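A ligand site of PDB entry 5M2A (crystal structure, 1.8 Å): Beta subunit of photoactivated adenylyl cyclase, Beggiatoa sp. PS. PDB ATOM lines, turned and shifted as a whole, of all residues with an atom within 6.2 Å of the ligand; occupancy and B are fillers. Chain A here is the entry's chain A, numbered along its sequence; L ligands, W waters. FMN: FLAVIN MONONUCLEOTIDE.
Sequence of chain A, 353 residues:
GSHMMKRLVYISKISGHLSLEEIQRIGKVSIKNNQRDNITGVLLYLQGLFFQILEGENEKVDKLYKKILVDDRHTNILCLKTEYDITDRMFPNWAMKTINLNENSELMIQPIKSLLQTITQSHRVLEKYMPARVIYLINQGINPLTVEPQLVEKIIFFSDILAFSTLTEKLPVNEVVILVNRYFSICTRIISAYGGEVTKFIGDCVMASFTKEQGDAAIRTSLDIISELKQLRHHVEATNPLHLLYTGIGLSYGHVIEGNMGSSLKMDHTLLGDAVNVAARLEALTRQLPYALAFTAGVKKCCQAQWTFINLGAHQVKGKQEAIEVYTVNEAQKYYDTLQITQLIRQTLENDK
OD2 of Asp 71 is in hydrogen-bond range of O2' of the ligand, at 2.8 Å. The side-chain amino group of Lys 67 lies within hydrogen-bond range of an oxygen (O4') of the ligand (3.4 Å). The guanidinium group (NH2) of Arg 73 sits at hydrogen-bond distance from an oxygen (O3') of the ligand (3.2 Å). An oxygen (O2) of the ligand is in hydrogen-bond range of the side-chain amide nitrogen (ND2) of Asn 33 (3.0 Å). N5 of the ligand lies close to OG of Ser 30, at 3.5 Å. NE2 of Gln 52 is in hydrogen-bond range of O4 of the ligand. OD1 of Asn 34 is in hydrogen-bond range of N3 of the ligand (2.9 Å).
The backbone NH (N) of Phe 50 sits at hydrogen-bond distance from the backbone carbonyl oxygen (O) of Ser 12 (2.9 Å). The backbone carbonyl oxygen (O) of Ile 68 lies within hydrogen-bond range of a ring nitrogen (NE2) of His 74 (2.8 Å). The backbone carbonyl oxygen (O) of Asn 34 sits at hydrogen-bond distance from the backbone NH (N) of Ile 39. The side-chain hydroxyl of Ser 12 is in hydrogen-bond range of a ring nitrogen (ND1) of His 74, 2.9 Å away. ND2 of Asn 34 sits at hydrogen-bond distance from O of Ala 95, 2.9 Å away. OD1 of Asn 34 sits close to O of Ser 30, at 3.2 Å. NE2 of Gln 52 lies close to SD of Met 96 (3.5 Å). The backbone carbonyl oxygen (O) of Ile 26 sits at hydrogen-bond distance from the side-chain hydroxyl (OG) of Ser 30, at 2.5 Å.
Residues that only touch the ligand: Leu 64 (3.3 Å), Tyr 10 (3.4 Å), Phe 50 (3.5 Å), Ile 26 (3.6 Å), Ile 68 (3.6 Å), Leu 54 (3.6 Å), Met 96 (3.8 Å), His 74 (3.9 Å), Val 29 (3.9 Å) and Leu 43 (3.9 Å). Hydrophobic or aromatic side chains within 4 Å of the ligand: Ile 26, Val 29, Leu 43, Phe 50, Leu 54, Leu 64, Ile 68, His 74 and Met 96. Within 4 Å of the ligand: Tyr 10, Ile 26, Val 29, Ser 30, Asn 33, Asn 34, Leu 43, Phe 50, Gln 52, Leu 54, Leu 64, Lys 67, Ile 68, Asp 71, Arg 73, His 74 and Met 96. The nearest printed residue that does not touch the ligand is Ser 12 (4.9 Å).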
ATOM      1  N   TYR A  10     -10.707 -33.147 -17.414  1.00  0.00           N
ATOM      2  CA  TYR A  10      -9.929 -32.942 -18.632  1.00  0.00           C
ATOM      3  C   TYR A  10      -9.359 -31.538 -18.635  1.00  0.00           C
ATOM      4  O   TYR A  10      -9.820 -30.645 -17.920  1.00  0.00           O
ATOM      5  CB  TYR A  10     -10.778 -33.178 -19.898  1.00  0.00           C
ATOM      6  CG  TYR A  10     -11.769 -32.082 -20.236  1.00  0.00           C
ATOM      7  CD1 TYR A  10     -11.372 -30.943 -20.920  1.00  0.00           C
ATOM      8  CD2 TYR A  10     -13.103 -32.209 -19.877  1.00  0.00           C
ATOM      9  CE1 TYR A  10     -12.290 -29.940 -21.223  1.00  0.00           C
ATOM     10  CE2 TYR A  10     -14.023 -31.219 -20.185  1.00  0.00           C
ATOM     11  CZ  TYR A  10     -13.600 -30.081 -20.850  1.00  0.00           C
ATOM     12  OH  TYR A  10     -14.507 -29.087 -21.154  1.00  0.00           O
ATOM     13  N   SER A  12      -7.803 -28.518 -21.592  1.00  0.00           N
ATOM     14  CA  SER A  12      -7.882 -28.148 -22.992  1.00  0.00           C
ATOM     15  C   SER A  12      -7.243 -26.787 -23.187  1.00  0.00           C
ATOM     16  O   SER A  12      -7.020 -26.034 -22.239  1.00  0.00           O
ATOM     17  CB  SER A  12      -9.333 -28.123 -23.486  1.00  0.00           C
ATOM     18  OG  SER A  12     -10.023 -27.024 -22.941  1.00  0.00           O
ATOM     19  N   LEU A  18     -10.630 -15.873 -26.206  1.00  0.00           N
ATOM     20  CA  LEU A  18     -12.056 -16.050 -25.939  1.00  0.00           C
ATOM     21  C   LEU A  18     -12.518 -14.975 -24.952  1.00  0.00           C
ATOM     22  O   LEU A  18     -11.906 -14.804 -23.892  1.00  0.00           O
ATOM     23  CB  LEU A  18     -12.333 -17.441 -25.381  1.00  0.00           C
ATOM     24  CG  LEU A  18     -13.677 -18.087 -25.725  1.00  0.00           C
ATOM     25  CD1 LEU A  18     -13.852 -18.213 -27.231  1.00  0.00           C
ATOM     26  CD2 LEU A  18     -13.786 -19.454 -25.059  1.00  0.00           C
ATOM     27  N   ILE A  26     -20.839 -20.109 -22.152  1.00  0.00           N
ATOM     28  CA  ILE A  26     -20.661 -21.531 -21.869  1.00  0.00           C
ATOM     29  C   ILE A  26     -21.310 -21.885 -20.534  1.00  0.00           C
ATOM     30  O   ILE A  26     -21.936 -22.941 -20.398  1.00  0.00           O
ATOM     31  CB  ILE A  26     -19.171 -21.893 -21.902  1.00  0.00           C
ATOM     32  CG1 ILE A  26     -18.569 -21.553 -23.270  1.00  0.00           C
ATOM     33  CG2 ILE A  26     -18.967 -23.364 -21.592  1.00  0.00           C
ATOM     34  CD1 ILE A  26     -17.079 -21.735 -23.343  1.00  0.00           C
ATOM     35  N   VAL A  29     -25.449 -22.075 -20.567  1.00  0.00           N
ATOM     36  CA  VAL A  29     -25.907 -23.248 -21.315  1.00  0.00           C
ATOM     37  C   VAL A  29     -25.521 -24.520 -20.568  1.00  0.00           C
ATOM     38  O   VAL A  29     -26.311 -25.473 -20.490  1.00  0.00           O
ATOM     39  CB  VAL A  29     -25.336 -23.235 -22.750  1.00  0.00           C
ATOM     40  CG1 VAL A  29     -25.609 -24.564 -23.440  1.00  0.00           C
ATOM     41  CG2 VAL A  29     -25.957 -22.102 -23.559  1.00  0.00           C
ATOM     42  N   SER A  30     -24.306 -24.555 -20.007  1.00  0.00           N
ATOM     43  CA  SER A  30     -23.904 -25.710 -19.211  1.00  0.00           C
ATOM     44  C   SER A  30     -24.817 -25.884 -18.006  1.00  0.00           C
ATOM     45  O   SER A  30     -25.292 -26.999 -17.737  1.00  0.00           O
ATOM     46  CB  SER A  30     -22.444 -25.553 -18.767  1.00  0.00           C
ATOM     47  OG  SER A  30     -21.600 -25.356 -19.892  1.00  0.00           O
ATOM     48  N   ILE A  31     -25.090 -24.807 -17.281  1.00  0.00           N
ATOM     49  CA  ILE A  31     -25.965 -24.880 -16.115  1.00  0.00           C
ATOM     50  C   ILE A  31     -27.342 -25.402 -16.506  1.00  0.00           C
ATOM     51  O   ILE A  31     -27.915 -26.257 -15.818  1.00  0.00           O
ATOM     52  CB  ILE A  31     -26.058 -23.499 -15.423  1.00  0.00           C
ATOM     53  CG1 ILE A  31     -24.730 -23.146 -14.775  1.00  0.00           C
ATOM     54  CG2 ILE A  31     -27.171 -23.499 -14.386  1.00  0.00           C
ATOM     55  CD1 ILE A  31     -24.721 -21.768 -14.141  1.00  0.00           C
ATOM     56  N   ASN A  33     -28.257 -27.225 -19.297  1.00  0.00           N
ATOM     57  CA  ASN A  33     -28.216 -28.611 -19.748  1.00  0.00           C
ATOM     58  C   ASN A  33     -27.866 -29.547 -18.598  1.00  0.00           C
ATOM     59  O   ASN A  33     -28.496 -30.608 -18.446  1.00  0.00           O
ATOM     60  CB  ASN A  33     -27.210 -28.754 -20.887  1.00  0.00           C
ATOM     61  CG  ASN A  33     -27.616 -27.997 -22.133  1.00  0.00           C
ATOM     62  OD1 ASN A  33     -28.745 -27.523 -22.249  1.00  0.00           O
ATOM     63  ND2 ASN A  33     -26.689 -27.871 -23.077  1.00  0.00           N
ATOM     64  N   ASN A  34     -26.890 -29.176 -17.770  1.00  0.00           N
ATOM     65  CA  ASN A  34     -26.452 -30.075 -16.706  1.00  0.00           C
ATOM     66  C   ASN A  34     -27.534 -30.271 -15.653  1.00  0.00           C
ATOM     67  O   ASN A  34     -27.645 -31.354 -15.067  1.00  0.00           O
ATOM     68  CB  ASN A  34     -25.160 -29.544 -16.064  1.00  0.00           C
ATOM     69  CG  ASN A  34     -23.985 -29.581 -17.031  1.00  0.00           C
ATOM     70  OD1 ASN A  34     -24.146 -29.900 -18.205  1.00  0.00           O
ATOM     71  ND2 ASN A  34     -22.801 -29.241 -16.526  1.00  0.00           N
ATOM     72  N   ARG A  36     -30.719 -30.351 -16.399  1.00  0.00           N
ATOM     73  CA  ARG A  36     -31.609 -31.315 -17.038  1.00  0.00           C
ATOM     74  C   ARG A  36     -31.039 -32.725 -16.948  1.00  0.00           C
ATOM     75  O   ARG A  36     -31.779 -33.676 -16.653  1.00  0.00           O
ATOM     76  CB  ARG A  36     -31.842 -30.926 -18.498  1.00  0.00           C
ATOM     77  CG  ARG A  36     -32.530 -31.991 -19.324  1.00  0.00           C
ATOM     78  CD  ARG A  36     -32.683 -31.554 -20.769  1.00  0.00           C
ATOM     79  NE  ARG A  36     -31.419 -31.089 -21.325  1.00  0.00           N
ATOM     80  CZ  ARG A  36     -30.489 -31.886 -21.846  1.00  0.00           C
ATOM     81  NH1 ARG A  36     -30.675 -33.198 -21.876  1.00  0.00           N
ATOM     82  NH2 ARG A  36     -29.363 -31.361 -22.326  1.00  0.00           N
ATOM     83  N   ASP A  37     -29.749 -32.875 -17.192  1.00  0.00           N
ATOM     84  CA  ASP A  37     -29.097 -34.183 -17.199  1.00  0.00           C
ATOM     85  C   ASP A  37     -28.607 -34.604 -15.816  1.00  0.00           C
ATOM     86  O   ASP A  37     -27.948 -35.643 -15.714  1.00  0.00           O
ATOM     87  CB  ASP A  37     -27.922 -34.185 -18.179  1.00  0.00           C
ATOM     88  CG  ASP A  37     -28.366 -34.094 -19.618  1.00  0.00           C
ATOM     89  OD1 ASP A  37     -29.494 -34.555 -19.920  1.00  0.00           O
ATOM     90  OD2 ASP A  37     -27.597 -33.565 -20.451  1.00  0.00           O
ATOM     91  N   ILE A  39     -26.252 -33.313 -14.147  1.00  0.00           N
ATOM     92  CA  ILE A  39     -24.791 -33.238 -14.196  1.00  0.00           C
ATOM     93  C   ILE A  39     -24.342 -32.093 -13.304  1.00  0.00           C
ATOM     94  O   ILE A  39     -24.980 -31.029 -13.269  1.00  0.00           O
ATOM     95  CB  ILE A  39     -24.281 -33.068 -15.636  1.00  0.00           C
ATOM     96  CG1 ILE A  39     -24.607 -34.311 -16.471  1.00  0.00           C
ATOM     97  CG2 ILE A  39     -22.765 -32.800 -15.671  1.00  0.00           C
ATOM     98  CD1 ILE A  39     -24.157 -34.223 -17.902  1.00  0.00           C
ATOM     99  N   LEU A  43     -15.840 -25.578 -13.956  1.00  0.00           N
ATOM    100  CA  LEU A  43     -15.046 -25.187 -15.109  1.00  0.00           C
ATOM    101  C   LEU A  43     -14.122 -24.065 -14.671  1.00  0.00           C
ATOM    102  O   LEU A  43     -14.598 -22.993 -14.292  1.00  0.00           O
ATOM    103  CB  LEU A  43     -15.935 -24.741 -16.275  1.00  0.00           C
ATOM    104  CG  LEU A  43     -15.225 -24.200 -17.515  1.00  0.00           C
ATOM    105  CD1 LEU A  43     -14.362 -25.288 -18.155  1.00  0.00           C
ATOM    106  CD2 LEU A  43     -16.236 -23.638 -18.509  1.00  0.00           C
ATOM    107  N   PHE A  50      -8.367 -24.447 -20.205  1.00  0.00           N
ATOM    108  CA  PHE A  50      -9.588 -24.845 -19.531  1.00  0.00           C
ATOM    109  C   PHE A  50      -9.309 -26.084 -18.678  1.00  0.00           C
ATOM    110  O   PHE A  50      -8.537 -26.957 -19.074  1.00  0.00           O
ATOM    111  CB  PHE A  50     -10.704 -25.176 -20.527  1.00  0.00           C
ATOM    112  CG  PHE A  50     -11.432 -23.979 -21.084  1.00  0.00           C
ATOM    113  CD1 PHE A  50     -11.855 -22.955 -20.261  1.00  0.00           C
ATOM    114  CD2 PHE A  50     -11.717 -23.902 -22.435  1.00  0.00           C
ATOM    115  CE1 PHE A  50     -12.539 -21.867 -20.776  1.00  0.00           C
ATOM    116  CE2 PHE A  50     -12.403 -22.817 -22.964  1.00  0.00           C
ATOM    117  CZ  PHE A  50     -12.813 -21.798 -22.127  1.00  0.00           C
ATOM    118  N   GLN A  52     -11.887 -28.835 -16.609  1.00  0.00           N
ATOM    119  CA  GLN A  52     -13.276 -29.107 -16.273  1.00  0.00           C
ATOM    120  C   GLN A  52     -13.429 -30.452 -15.596  1.00  0.00           C
ATOM    121  O   GLN A  52     -12.788 -31.430 -15.982  1.00  0.00           O
ATOM    122  CB  GLN A  52     -14.198 -29.026 -17.505  1.00  0.00           C
ATOM    123  CG  GLN A  52     -15.700 -28.928 -17.102  1.00  0.00           C
ATOM    124  CD  GLN A  52     -16.618 -28.652 -18.269  1.00  0.00           C
ATOM    125  OE1 GLN A  52     -16.301 -28.967 -19.416  1.00  0.00           O
ATOM    126  NE2 GLN A  52     -17.771 -28.054 -17.983  1.00  0.00           N
ATOM    127  N   LEU A  54     -16.571 -33.056 -14.645  1.00  0.00           N
ATOM    128  CA  LEU A  54     -17.960 -33.407 -14.919  1.00  0.00           C
ATOM    129  C   LEU A  54     -18.327 -34.651 -14.134  1.00  0.00           C
ATOM    130  O   LEU A  54     -17.536 -35.582 -14.028  1.00  0.00           O
ATOM    131  CB  LEU A  54     -18.179 -33.651 -16.419  1.00  0.00           C
ATOM    132  CG  LEU A  54     -17.937 -32.500 -17.400  1.00  0.00           C
ATOM    133  CD1 LEU A  54     -18.056 -33.005 -18.845  1.00  0.00           C
ATOM    134  CD2 LEU A  54     -18.921 -31.362 -17.151  1.00  0.00           C
ATOM    135  N   LEU A  64     -22.460 -35.827 -23.010  1.00  0.00           N
ATOM    136  CA  LEU A  64     -21.992 -34.444 -22.949  1.00  0.00           C
ATOM    137  C   LEU A  64     -20.542 -34.326 -23.398  1.00  0.00           C
ATOM    138  O   LEU A  64     -20.188 -33.386 -24.125  1.00  0.00           O
ATOM    139  CB  LEU A  64     -22.162 -33.913 -21.530  1.00  0.00           C
ATOM    140  CG  LEU A  64     -21.495 -32.566 -21.224  1.00  0.00           C
ATOM    141  CD1 LEU A  64     -22.003 -31.502 -22.161  1.00  0.00           C
ATOM    142  CD2 LEU A  64     -21.717 -32.178 -19.770  1.00  0.00           C
ATOM    143  N   LYS A  67     -19.985 -34.143 -27.050  1.00  0.00           N
ATOM    144  CA  LYS A  67     -20.269 -32.832 -27.631  1.00  0.00           C
ATOM    145  C   LYS A  67     -19.174 -31.833 -27.313  1.00  0.00           C
ATOM    146  O   LYS A  67     -18.769 -31.046 -28.173  1.00  0.00           O
ATOM    147  CB  LYS A  67     -21.614 -32.310 -27.126  1.00  0.00           C
ATOM    148  CG  LYS A  67     -22.769 -33.274 -27.340  1.00  0.00           C
ATOM    149  CD  LYS A  67     -24.070 -32.643 -26.877  1.00  0.00           C
ATOM    150  CE  LYS A  67     -23.897 -32.016 -25.491  1.00  0.00           C
ATOM    151  NZ  LYS A  67     -25.185 -31.502 -24.957  1.00  0.00           N
ATOM    152  N   ILE A  68     -18.680 -31.839 -26.065  1.00  0.00           N
ATOM    153  CA  ILE A  68     -17.597 -30.941 -25.690  1.00  0.00           C
ATOM    154  C   ILE A  68     -16.390 -31.175 -26.597  1.00  0.00           C
ATOM    155  O   ILE A  68     -15.719 -30.208 -27.007  1.00  0.00           O
ATOM    156  CB  ILE A  68     -17.243 -31.131 -24.205  1.00  0.00           C
ATOM    157  CG1 ILE A  68     -18.386 -30.643 -23.311  1.00  0.00           C
ATOM    158  CG2 ILE A  68     -15.966 -30.398 -23.860  1.00  0.00           C
ATOM    159  CD1 ILE A  68     -18.094 -30.799 -21.823  1.00  0.00           C
ATOM    160  N   LEU A  69     -16.119 -32.431 -26.940  1.00  0.00           N
ATOM    161  CA  LEU A  69     -14.949 -32.776 -27.755  1.00  0.00           C
ATOM    162  C   LEU A  69     -14.969 -32.066 -29.110  1.00  0.00           C
ATOM    163  O   LEU A  69     -13.911 -31.725 -29.648  1.00  0.00           O
ATOM    164  CB  LEU A  69     -14.875 -34.291 -27.955  1.00  0.00           C
ATOM    165  CG  LEU A  69     -14.258 -35.140 -26.841  1.00  0.00           C
ATOM    166  CD1 LEU A  69     -14.466 -36.618 -27.143  1.00  0.00           C
ATOM    167  CD2 LEU A  69     -12.777 -34.829 -26.690  1.00  0.00           C
ATOM    168  N   VAL A  70     -16.157 -31.863 -29.684  1.00  0.00           N
ATOM    169  CA  VAL A  70     -16.256 -31.235 -30.997  1.00  0.00           C
ATOM    170  C   VAL A  70     -16.553 -29.747 -30.882  1.00  0.00           C
ATOM    171  O   VAL A  70     -16.830 -29.095 -31.903  1.00  0.00           O
ATOM    172  CB  VAL A  70     -17.306 -31.957 -31.860  1.00  0.00           C
ATOM    173  CG1 VAL A  70     -17.006 -31.762 -33.345  1.00  0.00           C
ATOM    174  CG2 VAL A  70     -17.334 -33.445 -31.533  1.00  0.00           C
ATOM    175  N   ASP A  71     -16.481 -29.180 -29.688  1.00  0.00           N
ATOM    176  CA  ASP A  71     -16.720 -27.746 -29.520  1.00  0.00           C
ATOM    177  C   ASP A  71     -15.578 -26.945 -30.147  1.00  0.00           C
ATOM    178  O   ASP A  71     -14.401 -27.236 -29.941  1.00  0.00           O
ATOM    179  CB  ASP A  71     -16.869 -27.403 -28.040  1.00  0.00           C
ATOM    180  CG  ASP A  71     -17.504 -26.031 -27.815  1.00  0.00           C
ATOM    181  OD1 ASP A  71     -16.878 -25.017 -28.176  1.00  0.00           O
ATOM    182  OD2 ASP A  71     -18.631 -25.976 -27.273  1.00  0.00           O
ATOM    183  N   ARG A  73     -14.536 -24.036 -29.494  1.00  0.00           N
ATOM    184  CA  ARG A  73     -13.923 -23.025 -28.646  1.00  0.00           C
ATOM    185  C   ARG A  73     -12.699 -23.530 -27.884  1.00  0.00           C
ATOM    186  O   ARG A  73     -12.067 -22.751 -27.172  1.00  0.00           O
ATOM    187  CB  ARG A  73     -14.963 -22.471 -27.664  1.00  0.00           C
ATOM    188  CG  ARG A  73     -15.997 -21.568 -28.338  1.00  0.00           C
ATOM    189  CD  ARG A  73     -17.210 -21.294 -27.438  1.00  0.00           C
ATOM    190  NE  ARG A  73     -18.106 -22.439 -27.367  1.00  0.00           N
ATOM    191  CZ  ARG A  73     -19.342 -22.399 -26.886  1.00  0.00           C
ATOM    192  NH1 ARG A  73     -19.840 -21.252 -26.437  1.00  0.00           N
ATOM    193  NH2 ARG A  73     -20.097 -23.494 -26.861  1.00  0.00           N
ATOM    194  N   HIS A  74     -12.341 -24.803 -28.027  1.00  0.00           N
ATOM    195  CA  HIS A  74     -11.121 -25.286 -27.414  1.00  0.00           C
ATOM    196  C   HIS A  74     -10.550 -26.433 -28.245  1.00  0.00           C
ATOM    197  O   HIS A  74     -11.212 -26.986 -29.126  1.00  0.00           O
ATOM    198  CB  HIS A  74     -11.348 -25.692 -25.946  1.00  0.00           C
ATOM    199  CG  HIS A  74     -12.308 -26.820 -25.759  1.00  0.00           C
ATOM    200  ND1 HIS A  74     -12.363 -27.556 -24.591  1.00  0.00           N
ATOM    201  CD2 HIS A  74     -13.252 -27.340 -26.580  1.00  0.00           C
ATOM    202  CE1 HIS A  74     -13.308 -28.476 -24.700  1.00  0.00           C
ATOM    203  NE2 HIS A  74     -13.861 -28.373 -25.891  1.00  0.00           N
ATOM    204  N   ALA A  95     -24.492 -27.179 -10.841  1.00  0.00           N
ATOM    205  CA  ALA A  95     -24.713 -27.729 -12.175  1.00  0.00           C
ATOM    206  C   ALA A  95     -23.487 -27.510 -13.051  1.00  0.00           C
ATOM    207  O   ALA A  95     -23.003 -28.433 -13.727  1.00  0.00           O
ATOM    208  CB  ALA A  95     -25.953 -27.107 -12.796  1.00  0.00           C
ATOM    209  N   MET A  96     -22.969 -26.283 -13.049  1.00  0.00           N
ATOM    210  CA  MET A  96     -21.655 -25.988 -13.625  1.00  0.00           C
ATOM    211  C   MET A  96     -21.150 -24.664 -13.065  1.00  0.00           C
ATOM    212  O   MET A  96     -21.605 -23.589 -13.489  1.00  0.00           O
ATOM    213  CB  MET A  96     -21.710 -25.952 -15.150  1.00  0.00           C
ATOM    214  CG  MET A  96     -20.351 -25.701 -15.805  1.00  0.00           C
ATOM    215  SD  MET A  96     -19.005 -26.659 -15.067  1.00  0.00           S
ATOM    216  CE  MET A  96     -19.602 -28.344 -15.263  1.00  0.00           C
HETATM  217  N1  FMN L   1     -22.199 -27.841 -22.458  1.00  0.00           N
HETATM  218  C2  FMN L   1     -22.965 -28.440 -21.467  1.00  0.00           C
HETATM  219  O2  FMN L   1     -24.139 -28.716 -21.687  1.00  0.00           O
HETATM  220  N3  FMN L   1     -22.408 -28.742 -20.247  1.00  0.00           N
HETATM  221  C4  FMN L   1     -21.089 -28.437 -19.997  1.00  0.00           C
HETATM  222  O4  FMN L   1     -20.584 -28.699 -18.900  1.00  0.00           O
HETATM  223  C4A FMN L   1     -20.316 -27.841 -20.981  1.00  0.00           C
HETATM  224  N5  FMN L   1     -19.000 -27.541 -20.715  1.00  0.00           N
HETATM  225  C5A FMN L   1     -18.231 -26.950 -21.683  1.00  0.00           C
HETATM  226  C6  FMN L   1     -16.907 -26.664 -21.401  1.00  0.00           C
HETATM  227  C7  FMN L   1     -16.109 -26.068 -22.367  1.00  0.00           C
HETATM  228  C7M FMN L   1     -14.672 -25.762 -22.041  1.00  0.00           C
HETATM  229  C8  FMN L   1     -16.647 -25.764 -23.619  1.00  0.00           C
HETATM  230  C8M FMN L   1     -15.800 -25.113 -24.668  1.00  0.00           C
HETATM  231  C9  FMN L   1     -17.976 -26.058 -23.899  1.00  0.00           C
HETATM  232  C9A FMN L   1     -18.768 -26.656 -22.926  1.00  0.00           C
HETATM  233  N10 FMN L   1     -20.091 -26.953 -23.199  1.00  0.00           N
HETATM  234  C10 FMN L   1     -20.870 -27.547 -22.222  1.00  0.00           C
HETATM  235  C1' FMN L   1     -20.658 -26.591 -24.544  1.00  0.00           C
HETATM  236  C2' FMN L   1     -21.040 -27.789 -25.408  1.00  0.00           C
HETATM  237  O2' FMN L   1     -19.916 -28.188 -26.170  1.00  0.00           O
HETATM  238  C3' FMN L   1     -22.171 -27.379 -26.349  1.00  0.00           C
HETATM  239  O3' FMN L   1     -21.820 -26.149 -26.962  1.00  0.00           O
HETATM  240  C4' FMN L   1     -23.469 -27.206 -25.570  1.00  0.00           C
HETATM  241  O4' FMN L   1     -23.792 -28.411 -24.929  1.00  0.00           O
HETATM  242  C5' FMN L   1     -24.614 -26.803 -26.485  1.00  0.00           C
HETATM  243  O5' FMN L   1     -24.795 -27.810 -27.451  1.00  0.00           O
HETATM  244  P   FMN L   1     -26.087 -27.809 -28.408  1.00  0.00           P
HETATM  245  O1P FMN L   1     -27.246 -28.375 -27.632  1.00  0.00           O
HETATM  246  O2P FMN L   1     -26.396 -26.395 -28.829  1.00  0.00           O
HETATM  247  O3P FMN L   1     -25.804 -28.668 -29.625  1.00  0.00           O
HETATM  248  O   HOH W   1     -25.165 -31.209 -20.507  1.00  0.00           O
HETATM  249  O   HOH W   2     -26.353 -23.804 -27.717  1.00  0.00           O
